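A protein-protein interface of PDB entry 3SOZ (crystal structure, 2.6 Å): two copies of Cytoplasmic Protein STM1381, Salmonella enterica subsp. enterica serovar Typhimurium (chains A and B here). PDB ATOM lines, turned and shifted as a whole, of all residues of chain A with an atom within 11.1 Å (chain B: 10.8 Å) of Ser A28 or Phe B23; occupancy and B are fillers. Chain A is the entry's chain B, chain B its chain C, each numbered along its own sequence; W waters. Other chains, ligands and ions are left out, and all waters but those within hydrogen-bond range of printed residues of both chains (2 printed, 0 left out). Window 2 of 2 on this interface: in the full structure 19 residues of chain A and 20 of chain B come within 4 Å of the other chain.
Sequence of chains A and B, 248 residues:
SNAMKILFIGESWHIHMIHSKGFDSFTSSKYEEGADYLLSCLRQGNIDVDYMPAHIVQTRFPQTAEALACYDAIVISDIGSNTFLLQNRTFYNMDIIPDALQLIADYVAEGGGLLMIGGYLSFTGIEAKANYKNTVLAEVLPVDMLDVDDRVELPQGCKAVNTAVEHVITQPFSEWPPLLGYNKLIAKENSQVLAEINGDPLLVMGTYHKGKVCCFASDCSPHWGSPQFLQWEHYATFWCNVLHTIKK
Water W2 lies within hydrogen-bond range of the side-chain hydroxyl (OG) of Ser A29 (2.5 Å), the side-chain hydroxyl (OG) of Ser B25 (2.6 Å), the backbone carbonyl oxygen (O) of Phe B23 (2.7 Å) and the side-chain hydroxyl (OG1) of Thr A27 (2.8 Å).
Water W1 lies within hydrogen-bond range of OH of Tyr A31 (2.9 Å), NE2 of His A14 (3.0 Å) and O of Gly B22 (3.1 Å).
A ring nitrogen (ND1) of His A16 is in hydrogen-bond range of the side-chain hydroxyl (OG) of Ser A29, at 3.1 Å.
O of Ser A28 sits at hydrogen-bond distance from N of Met A17 (2.7 Å).
The side-chain hydroxyl (OG) of Ser A28 sits close to a ring nitrogen (NE2) of His A19 (3.5 Å).
The side-chain hydroxyl of Ser B25 lies within hydrogen-bond range of the side-chain hydroxyl of Ser B20, at 2.9 Å.
Among the printed residues, pairs that only touch across the chains: His A14 with Ser B20 (3.5 Å), Ser A28 with Phe B23 (3.6 Å), His A16 with Ile B18 (3.6 Å), Thr A27 with Phe B23 (3.7 Å) and Thr A27 with Ser B25 (3.9 Å).
The side-chain hydroxyl (OG) of Ser B20 sits at hydrogen-bond distance from a ring nitrogen (ND1) of His A16 (3.5 Å).
A ring nitrogen (ND1) of His A16 lies close to the side-chain hydroxyl of Ser B25 (3.3 Å).
OG of Ser B20 sits at hydrogen-bond distance from OG of Ser A29, 3.4 Å away.
N of Ser A29 is in hydrogen-bond range of O of Phe B23 (3.0 Å).
OG of Ser A29 sits at hydrogen-bond distance from OG of Ser B25 (3.3 Å).
The side-chain hydroxyl (OH) of Tyr A31 sits at hydrogen-bond distance from the backbone NH (N) of Gly B22 (3.2 Å).
The backbone carbonyl oxygen of Ser A29 lies close to the backbone carbonyl oxygen of Gly B22 (3.2 Å).
Of chain B, only Phe B23 (3.6 Å) comes within 4 Å of Ser A28.
Phe B23 touches three residues of chain A.
No residue of chain B comes within 4 Å of Met A17.
Of chain B, only Phe B23 and Ser B25 come within 4 Å of Thr A27.
Asp B24 touches none of the printed residues of chain A.
Printed residues of chain A within 4 Å of Ser B20: His A14 (3.5 Å), His A16 (3.5 Å) and Ser A29 (3.4 Å).
Printed residues of chain B within 4 Å of Tyr A31: Gly B22.
His A19 touches none of the printed residues of chain B.
The nearest residue of chain B that does not touch Ser A28 is Gly B22 (5.5 Å).
The nearest printed residue of chain B that does not touch His A14 is Gly B22 (5.6 Å).
5 positions are printed for both chains.
Of the 12 pairs that touch across the chains among the printed residues, none has its exchanged pair printed and touching as well.
Of the 9 printed residues of chain B, 5 touch a printed residue of chain A.
Hydrophobic or aromatic side chains of chain B within 4 Å of the printed part of chain A: Ile B18 and Phe B23.
Of the 16 printed residues of chain A, 6 touch a printed residue of chain B.
Hydrophobic or aromatic side chains of chain A that line the printed part of chain B: His A14, His A16 and Tyr A31.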
ATOM      1  N   TRP A  13       4.610 -27.909  -1.703  1.00  0.00           N
ATOM      2  CA  TRP A  13       4.118 -26.535  -1.725  1.00  0.00           C
ATOM      3  C   TRP A  13       3.275 -26.388  -2.941  1.00  0.00           C
ATOM      4  O   TRP A  13       3.701 -26.882  -3.994  1.00  0.00           O
ATOM      5  CB  TRP A  13       5.309 -25.609  -1.841  1.00  0.00           C
ATOM      6  CG  TRP A  13       5.968 -25.396  -0.525  1.00  0.00           C
ATOM      7  CD1 TRP A  13       7.130 -25.943  -0.076  1.00  0.00           C
ATOM      8  CD2 TRP A  13       5.490 -24.544   0.522  1.00  0.00           C
ATOM      9  NE1 TRP A  13       7.404 -25.488   1.184  1.00  0.00           N
ATOM     10  CE2 TRP A  13       6.415 -24.627   1.576  1.00  0.00           C
ATOM     11  CE3 TRP A  13       4.362 -23.722   0.665  1.00  0.00           C
ATOM     12  CZ2 TRP A  13       6.261 -23.913   2.763  1.00  0.00           C
ATOM     13  CZ3 TRP A  13       4.196 -23.030   1.837  1.00  0.00           C
ATOM     14  CH2 TRP A  13       5.152 -23.121   2.877  1.00  0.00           C
ATOM     15  N   HIS A  14       2.099 -25.762  -2.829  1.00  0.00           N
ATOM     16  CA  HIS A  14       1.350 -25.363  -4.024  1.00  0.00           C
ATOM     17  C   HIS A  14       1.821 -23.939  -4.406  1.00  0.00           C
ATOM     18  O   HIS A  14       2.078 -23.151  -3.526  1.00  0.00           O
ATOM     19  CB  HIS A  14      -0.194 -25.402  -3.832  1.00  0.00           C
ATOM     20  CG  HIS A  14      -0.912 -24.845  -5.007  1.00  0.00           C
ATOM     21  ND1 HIS A  14      -1.114 -23.494  -5.164  1.00  0.00           N
ATOM     22  CD2 HIS A  14      -1.289 -25.418  -6.172  1.00  0.00           C
ATOM     23  CE1 HIS A  14      -1.647 -23.260  -6.352  1.00  0.00           C
ATOM     24  NE2 HIS A  14      -1.756 -24.413  -6.986  1.00  0.00           N
ATOM     25  N   ILE A  15       1.935 -23.589  -5.676  1.00  0.00           N
ATOM     26  CA  ILE A  15       2.446 -22.255  -6.033  1.00  0.00           C
ATOM     27  C   ILE A  15       1.483 -21.569  -6.923  1.00  0.00           C
ATOM     28  O   ILE A  15       1.103 -22.110  -7.956  1.00  0.00           O
ATOM     29  CB  ILE A  15       3.860 -22.276  -6.781  1.00  0.00           C
ATOM     30  CG1 ILE A  15       4.895 -23.045  -5.955  1.00  0.00           C
ATOM     31  CG2 ILE A  15       4.360 -20.906  -7.017  1.00  0.00           C
ATOM     32  CD1 ILE A  15       5.488 -22.311  -4.843  1.00  0.00           C
ATOM     33  N   HIS A  16       1.044 -20.392  -6.504  1.00  0.00           N
ATOM     34  CA  HIS A  16       0.117 -19.642  -7.350  1.00  0.00           C
ATOM     35  C   HIS A  16       0.713 -18.335  -7.710  1.00  0.00           C
ATOM     36  O   HIS A  16       1.096 -17.573  -6.825  1.00  0.00           O
ATOM     37  CB  HIS A  16      -1.277 -19.481  -6.711  1.00  0.00           C
ATOM     38  CG  HIS A  16      -2.200 -18.630  -7.524  1.00  0.00           C
ATOM     39  ND1 HIS A  16      -2.901 -19.121  -8.604  1.00  0.00           N
ATOM     40  CD2 HIS A  16      -2.494 -17.308  -7.457  1.00  0.00           C
ATOM     41  CE1 HIS A  16      -3.600 -18.143  -9.162  1.00  0.00           C
ATOM     42  NE2 HIS A  16      -3.376 -17.036  -8.479  1.00  0.00           N
ATOM     43  N   MET A  17       0.815 -18.083  -9.005  1.00  0.00           N
ATOM     44  CA  MET A  17       1.641 -16.974  -9.477  1.00  0.00           C
ATOM     45  C   MET A  17       0.823 -15.952 -10.191  1.00  0.00           C
ATOM     46  O   MET A  17       0.225 -16.260 -11.217  1.00  0.00           O
ATOM     47  CB  MET A  17       2.747 -17.529 -10.389  1.00  0.00           C
ATOM     48  CG  MET A  17       4.055 -16.789 -10.382  1.00  0.00           C
ATOM     49  SD  MET A  17       5.614 -17.821 -11.214  1.00  0.00           S
ATOM     50  CE  MET A  17       5.624 -19.299  -9.952  1.00  0.00           C
ATOM     51  N   ILE A  18       0.740 -14.750  -9.634  1.00  0.00           N
ATOM     52  CA  ILE A  18       0.069 -13.634 -10.331  1.00  0.00           C
ATOM     53  C   ILE A  18       1.126 -12.845 -11.090  1.00  0.00           C
ATOM     54  O   ILE A  18       2.120 -12.434 -10.471  1.00  0.00           O
ATOM     55  CB  ILE A  18      -0.674 -12.708  -9.347  1.00  0.00           C
ATOM     56  CG1 ILE A  18      -1.715 -13.491  -8.547  1.00  0.00           C
ATOM     57  CG2 ILE A  18      -1.338 -11.518 -10.050  1.00  0.00           C
ATOM     58  CD1 ILE A  18      -1.998 -12.879  -7.130  1.00  0.00           C
ATOM     59  N   HIS A  19       0.952 -12.695 -12.408  1.00  0.00           N
ATOM     60  CA  HIS A  19       1.879 -11.900 -13.240  1.00  0.00           C
ATOM     61  C   HIS A  19       1.205 -10.610 -13.737  1.00  0.00           C
ATOM     62  O   HIS A  19       0.232 -10.651 -14.561  1.00  0.00           O
ATOM     63  CB  HIS A  19       2.298 -12.633 -14.512  1.00  0.00           C
ATOM     64  CG  HIS A  19       2.855 -14.016 -14.322  1.00  0.00           C
ATOM     65  ND1 HIS A  19       2.114 -15.071 -13.829  1.00  0.00           N
ATOM     66  CD2 HIS A  19       4.044 -14.548 -14.712  1.00  0.00           C
ATOM     67  CE1 HIS A  19       2.844 -16.171 -13.855  1.00  0.00           C
ATOM     68  NE2 HIS A  19       4.018 -15.880 -14.390  1.00  0.00           N
ATOM     69  N   SER A  20       1.721  -9.476 -13.302  1.00  0.00           N
ATOM     70  CA  SER A  20       1.092  -8.170 -13.623  1.00  0.00           C
ATOM     71  C   SER A  20       1.942  -7.298 -14.523  1.00  0.00           C
ATOM     72  O   SER A  20       3.180  -7.239 -14.407  1.00  0.00           O
ATOM     73  CB  SER A  20       0.891  -7.386 -12.355  1.00  0.00           C
ATOM     74  OG  SER A  20       0.191  -8.139 -11.430  1.00  0.00           O
ATOM     75  N   SER A  25      -3.186  -8.527 -15.664  1.00  0.00           N
ATOM     76  CA  SER A  25      -2.569  -9.668 -14.967  1.00  0.00           C
ATOM     77  C   SER A  25      -2.958 -10.963 -15.601  1.00  0.00           C
ATOM     78  O   SER A  25      -4.081 -11.132 -16.121  1.00  0.00           O
ATOM     79  CB  SER A  25      -3.030  -9.719 -13.515  1.00  0.00           C
ATOM     80  OG  SER A  25      -2.427  -8.657 -12.754  1.00  0.00           O
ATOM     81  N   PHE A  26      -2.060 -11.922 -15.548  1.00  0.00           N
ATOM     82  CA  PHE A  26      -2.537 -13.307 -15.657  1.00  0.00           C
ATOM     83  C   PHE A  26      -1.878 -14.191 -14.607  1.00  0.00           C
ATOM     84  O   PHE A  26      -0.868 -13.801 -13.975  1.00  0.00           O
ATOM     85  CB  PHE A  26      -2.310 -13.837 -17.068  1.00  0.00           C
ATOM     86  CG  PHE A  26      -0.915 -14.257 -17.342  1.00  0.00           C
ATOM     87  CD1 PHE A  26       0.063 -13.322 -17.655  1.00  0.00           C
ATOM     88  CD2 PHE A  26      -0.582 -15.588 -17.334  1.00  0.00           C
ATOM     89  CE1 PHE A  26       1.386 -13.692 -17.913  1.00  0.00           C
ATOM     90  CE2 PHE A  26       0.716 -15.984 -17.586  1.00  0.00           C
ATOM     91  CZ  PHE A  26       1.713 -15.029 -17.863  1.00  0.00           C
ATOM     92  N   THR A  27      -2.393 -15.384 -14.410  1.00  0.00           N
ATOM     93  CA  THR A  27      -1.760 -16.249 -13.429  1.00  0.00           C
ATOM     94  C   THR A  27      -1.120 -17.500 -14.028  1.00  0.00           C
ATOM     95  O   THR A  27      -1.460 -17.943 -15.130  1.00  0.00           O
ATOM     96  CB  THR A  27      -2.760 -16.682 -12.318  1.00  0.00           C
ATOM     97  OG1 THR A  27      -3.657 -17.616 -12.876  1.00  0.00           O
ATOM     98  CG2 THR A  27      -3.581 -15.519 -11.817  1.00  0.00           C
ATOM     99  N   SER A  28      -0.190 -18.080 -13.298  1.00  0.00           N
ATOM    100  CA  SER A  28       0.241 -19.432 -13.610  1.00  0.00           C
ATOM    101  C   SER A  28       0.342 -20.162 -12.278  1.00  0.00           C
ATOM    102  O   SER A  28       0.580 -19.514 -11.259  1.00  0.00           O
ATOM    103  CB  SER A  28       1.560 -19.386 -14.375  1.00  0.00           C
ATOM    104  OG  SER A  28       2.666 -18.972 -13.559  1.00  0.00           O
ATOM    105  N   SER A  29       0.145 -21.469 -12.242  1.00  0.00           N
ATOM    106  CA  SER A  29       0.219 -22.249 -10.995  1.00  0.00           C
ATOM    107  C   SER A  29       1.000 -23.507 -11.185  1.00  0.00           C
ATOM    108  O   SER A  29       1.059 -24.081 -12.271  1.00  0.00           O
ATOM    109  CB  SER A  29      -1.210 -22.664 -10.514  1.00  0.00           C
ATOM    110  OG  SER A  29      -2.092 -21.544 -10.391  1.00  0.00           O
ATOM    111  N   LYS A  30       1.550 -24.002 -10.104  1.00  0.00           N
ATOM    112  CA  LYS A  30       2.244 -25.300 -10.115  1.00  0.00           C
ATOM    113  C   LYS A  30       2.526 -25.836  -8.709  1.00  0.00           C
ATOM    114  O   LYS A  30       2.031 -25.237  -7.767  1.00  0.00           O
ATOM    115  CB  LYS A  30       3.516 -25.226 -10.966  1.00  0.00           C
ATOM    116  CG  LYS A  30       4.256 -23.985 -10.818  1.00  0.00           C
ATOM    117  CD  LYS A  30       5.437 -24.257  -9.973  1.00  0.00           C
ATOM    118  CE  LYS A  30       6.710 -24.177 -10.737  1.00  0.00           C
ATOM    119  NZ  LYS A  30       7.550 -24.972  -9.823  1.00  0.00           N
ATOM    120  N   TYR A  31       3.236 -26.975  -8.581  1.00  0.00           N
ATOM    121  CA  TYR A  31       3.627 -27.562  -7.280  1.00  0.00           C
ATOM    122  C   TYR A  31       5.153 -27.726  -7.134  1.00  0.00           C
ATOM    123  O   TYR A  31       5.898 -27.453  -8.057  1.00  0.00           O
ATOM    124  CB  TYR A  31       2.886 -28.849  -7.011  1.00  0.00           C
ATOM    125  CG  TYR A  31       1.521 -28.824  -7.583  1.00  0.00           C
ATOM    126  CD1 TYR A  31       1.351 -28.736  -8.973  1.00  0.00           C
ATOM    127  CD2 TYR A  31       0.371 -28.880  -6.762  1.00  0.00           C
ATOM    128  CE1 TYR A  31       0.072 -28.695  -9.575  1.00  0.00           C
ATOM    129  CE2 TYR A  31      -0.933 -28.817  -7.331  1.00  0.00           C
ATOM    130  CZ  TYR A  31      -1.068 -28.733  -8.765  1.00  0.00           C
ATOM    131  OH  TYR A  31      -2.299 -28.694  -9.432  1.00  0.00           O
ATOM    132  N   GLU A  32       5.642 -28.121  -5.973  1.00  0.00           N
ATOM    133  CA  GLU A  32       7.067 -28.060  -5.807  1.00  0.00           C
ATOM    134  C   GLU A  32       7.780 -29.349  -5.499  1.00  0.00           C
ATOM    135  O   GLU A  32       8.991 -29.458  -5.746  1.00  0.00           O
ATOM    136  CB  GLU A  32       7.493 -26.918  -4.883  1.00  0.00           C
ATOM    137  CG  GLU A  32       7.836 -25.657  -5.676  1.00  0.00           C
ATOM    138  CD  GLU A  32       8.359 -24.491  -4.801  1.00  0.00           C
ATOM    139  OE1 GLU A  32       8.592 -24.688  -3.580  1.00  0.00           O
ATOM    140  OE2 GLU A  32       8.517 -23.361  -5.339  1.00  0.00           O
ATOM    141  N   ILE B  18      -9.516 -18.675  -4.814  1.00  0.00           N
ATOM    142  CA  ILE B  18      -8.717 -19.036  -5.951  1.00  0.00           C
ATOM    143  C   ILE B  18      -8.636 -20.561  -6.110  1.00  0.00           C
ATOM    144  O   ILE B  18      -8.075 -21.269  -5.281  1.00  0.00           O
ATOM    145  CB  ILE B  18      -7.328 -18.494  -5.821  1.00  0.00           C
ATOM    146  CG1 ILE B  18      -7.373 -16.981  -5.599  1.00  0.00           C
ATOM    147  CG2 ILE B  18      -6.485 -18.834  -7.124  1.00  0.00           C
ATOM    148  CD1 ILE B  18      -5.951 -16.341  -5.469  1.00  0.00           C
ATOM    149  N   HIS B  19      -9.231 -21.043  -7.190  1.00  0.00           N
ATOM    150  CA  HIS B  19      -9.228 -22.461  -7.548  1.00  0.00           C
ATOM    151  C   HIS B  19      -8.121 -22.700  -8.551  1.00  0.00           C
ATOM    152  O   HIS B  19      -8.059 -22.060  -9.636  1.00  0.00           O
ATOM    153  CB  HIS B  19     -10.585 -22.870  -8.132  1.00  0.00           C
ATOM    154  CG  HIS B  19     -11.767 -22.421  -7.305  1.00  0.00           C
ATOM    155  ND1 HIS B  19     -12.605 -23.300  -6.655  1.00  0.00           N
ATOM    156  CD2 HIS B  19     -12.248 -21.189  -7.030  1.00  0.00           C
ATOM    157  CE1 HIS B  19     -13.562 -22.642  -6.041  1.00  0.00           C
ATOM    158  NE2 HIS B  19     -13.362 -21.355  -6.240  1.00  0.00           N
ATOM    159  N   SER B  20      -7.228 -23.604  -8.209  1.00  0.00           N
ATOM    160  CA  SER B  20      -6.087 -23.860  -9.081  1.00  0.00           C
ATOM    161  C   SER B  20      -6.035 -25.294  -9.484  1.00  0.00           C
ATOM    162  O   SER B  20      -6.252 -26.191  -8.664  1.00  0.00           O
ATOM    163  CB  SER B  20      -4.786 -23.453  -8.373  1.00  0.00           C
ATOM    164  OG  SER B  20      -4.760 -22.028  -8.307  1.00  0.00           O
ATOM    165  N   LYS B  21      -5.783 -25.526 -10.761  1.00  0.00           N
ATOM    166  CA  LYS B  21      -5.410 -26.890 -11.192  1.00  0.00           C
ATOM    167  C   LYS B  21      -4.484 -26.866 -12.417  1.00  0.00           C
ATOM    168  O   LYS B  21      -4.810 -26.268 -13.473  1.00  0.00           O
ATOM    169  CB  LYS B  21      -6.645 -27.741 -11.466  1.00  0.00           C
ATOM    170  CG  LYS B  21      -6.329 -29.230 -11.383  1.00  0.00           C
ATOM    171  CD  LYS B  21      -7.439 -30.033 -11.974  1.00  0.00           C
ATOM    172  CE  LYS B  21      -8.735 -29.881 -11.228  1.00  0.00           C
ATOM    173  NZ  LYS B  21      -9.826 -30.649 -11.889  1.00  0.00           N
ATOM    174  N   GLY B  22      -3.324 -27.493 -12.246  1.00  0.00           N
ATOM    175  CA  GLY B  22      -2.258 -27.425 -13.232  1.00  0.00           C
ATOM    176  C   GLY B  22      -1.940 -25.967 -13.457  1.00  0.00           C
ATOM    177  O   GLY B  22      -1.964 -25.154 -12.541  1.00  0.00           O
ATOM    178  N   PHE B  23      -1.712 -25.595 -14.695  1.00  0.00           N
ATOM    179  CA  PHE B  23      -1.471 -24.190 -14.992  1.00  0.00           C
ATOM    180  C   PHE B  23      -2.494 -23.180 -14.480  1.00  0.00           C
ATOM    181  O   PHE B  23      -2.122 -22.109 -14.092  1.00  0.00           O
ATOM    182  CB  PHE B  23      -1.449 -23.997 -16.489  1.00  0.00           C
ATOM    183  CG  PHE B  23      -0.746 -22.777 -16.893  1.00  0.00           C
ATOM    184  CD1 PHE B  23       0.640 -22.731 -16.832  1.00  0.00           C
ATOM    185  CD2 PHE B  23      -1.446 -21.670 -17.304  1.00  0.00           C
ATOM    186  CE1 PHE B  23       1.330 -21.563 -17.223  1.00  0.00           C
ATOM    187  CE2 PHE B  23      -0.784 -20.509 -17.685  1.00  0.00           C
ATOM    188  CZ  PHE B  23       0.620 -20.466 -17.640  1.00  0.00           C
ATOM    189  N   ASP B  24      -3.779 -23.551 -14.519  1.00  0.00           N
ATOM    190  CA  ASP B  24      -4.879 -22.623 -14.549  1.00  0.00           C
ATOM    191  C   ASP B  24      -5.531 -22.354 -13.219  1.00  0.00           C
ATOM    192  O   ASP B  24      -5.557 -23.239 -12.302  1.00  0.00           O
ATOM    193  CB  ASP B  24      -5.927 -23.228 -15.459  1.00  0.00           C
ATOM    194  CG  ASP B  24      -5.444 -23.325 -16.888  1.00  0.00           C
ATOM    195  OD1 ASP B  24      -5.092 -22.249 -17.490  1.00  0.00           O
ATOM    196  OD2 ASP B  24      -5.402 -24.471 -17.405  1.00  0.00           O
ATOM    197  N   SER B  25      -6.114 -21.166 -13.114  1.00  0.00           N
ATOM    198  CA  SER B  25      -7.034 -20.837 -11.965  1.00  0.00           C
ATOM    199  C   SER B  25      -8.360 -20.252 -12.363  1.00  0.00           C
ATOM    200  O   SER B  25      -8.543 -19.613 -13.427  1.00  0.00           O
ATOM    201  CB  SER B  25      -6.376 -19.850 -11.057  1.00  0.00           C
ATOM    202  OG  SER B  25      -5.151 -20.383 -10.631  1.00  0.00           O
ATOM    203  N   PHE B  26      -9.327 -20.410 -11.515  1.00  0.00           N
ATOM    204  CA  PHE B  26     -10.422 -19.474 -11.689  1.00  0.00           C
ATOM    205  C   PHE B  26     -10.764 -19.082 -10.251  1.00  0.00           C
ATOM    206  O   PHE B  26     -10.250 -19.733  -9.280  1.00  0.00           O
ATOM    207  CB  PHE B  26     -11.591 -20.075 -12.478  1.00  0.00           C
ATOM    208  CG  PHE B  26     -12.383 -21.050 -11.690  1.00  0.00           C
ATOM    209  CD1 PHE B  26     -11.922 -22.381 -11.525  1.00  0.00           C
ATOM    210  CD2 PHE B  26     -13.593 -20.654 -11.096  1.00  0.00           C
ATOM    211  CE1 PHE B  26     -12.669 -23.332 -10.732  1.00  0.00           C
ATOM    212  CE2 PHE B  26     -14.366 -21.583 -10.328  1.00  0.00           C
ATOM    213  CZ  PHE B  26     -13.904 -22.927 -10.111  1.00  0.00           C
HETATM  214  O   HOH W   1      -2.161 -25.819  -9.552  1.00  0.00           O
HETATM  215  O   HOH W   2      -3.135 -20.355 -12.319  1.00  0.00           O
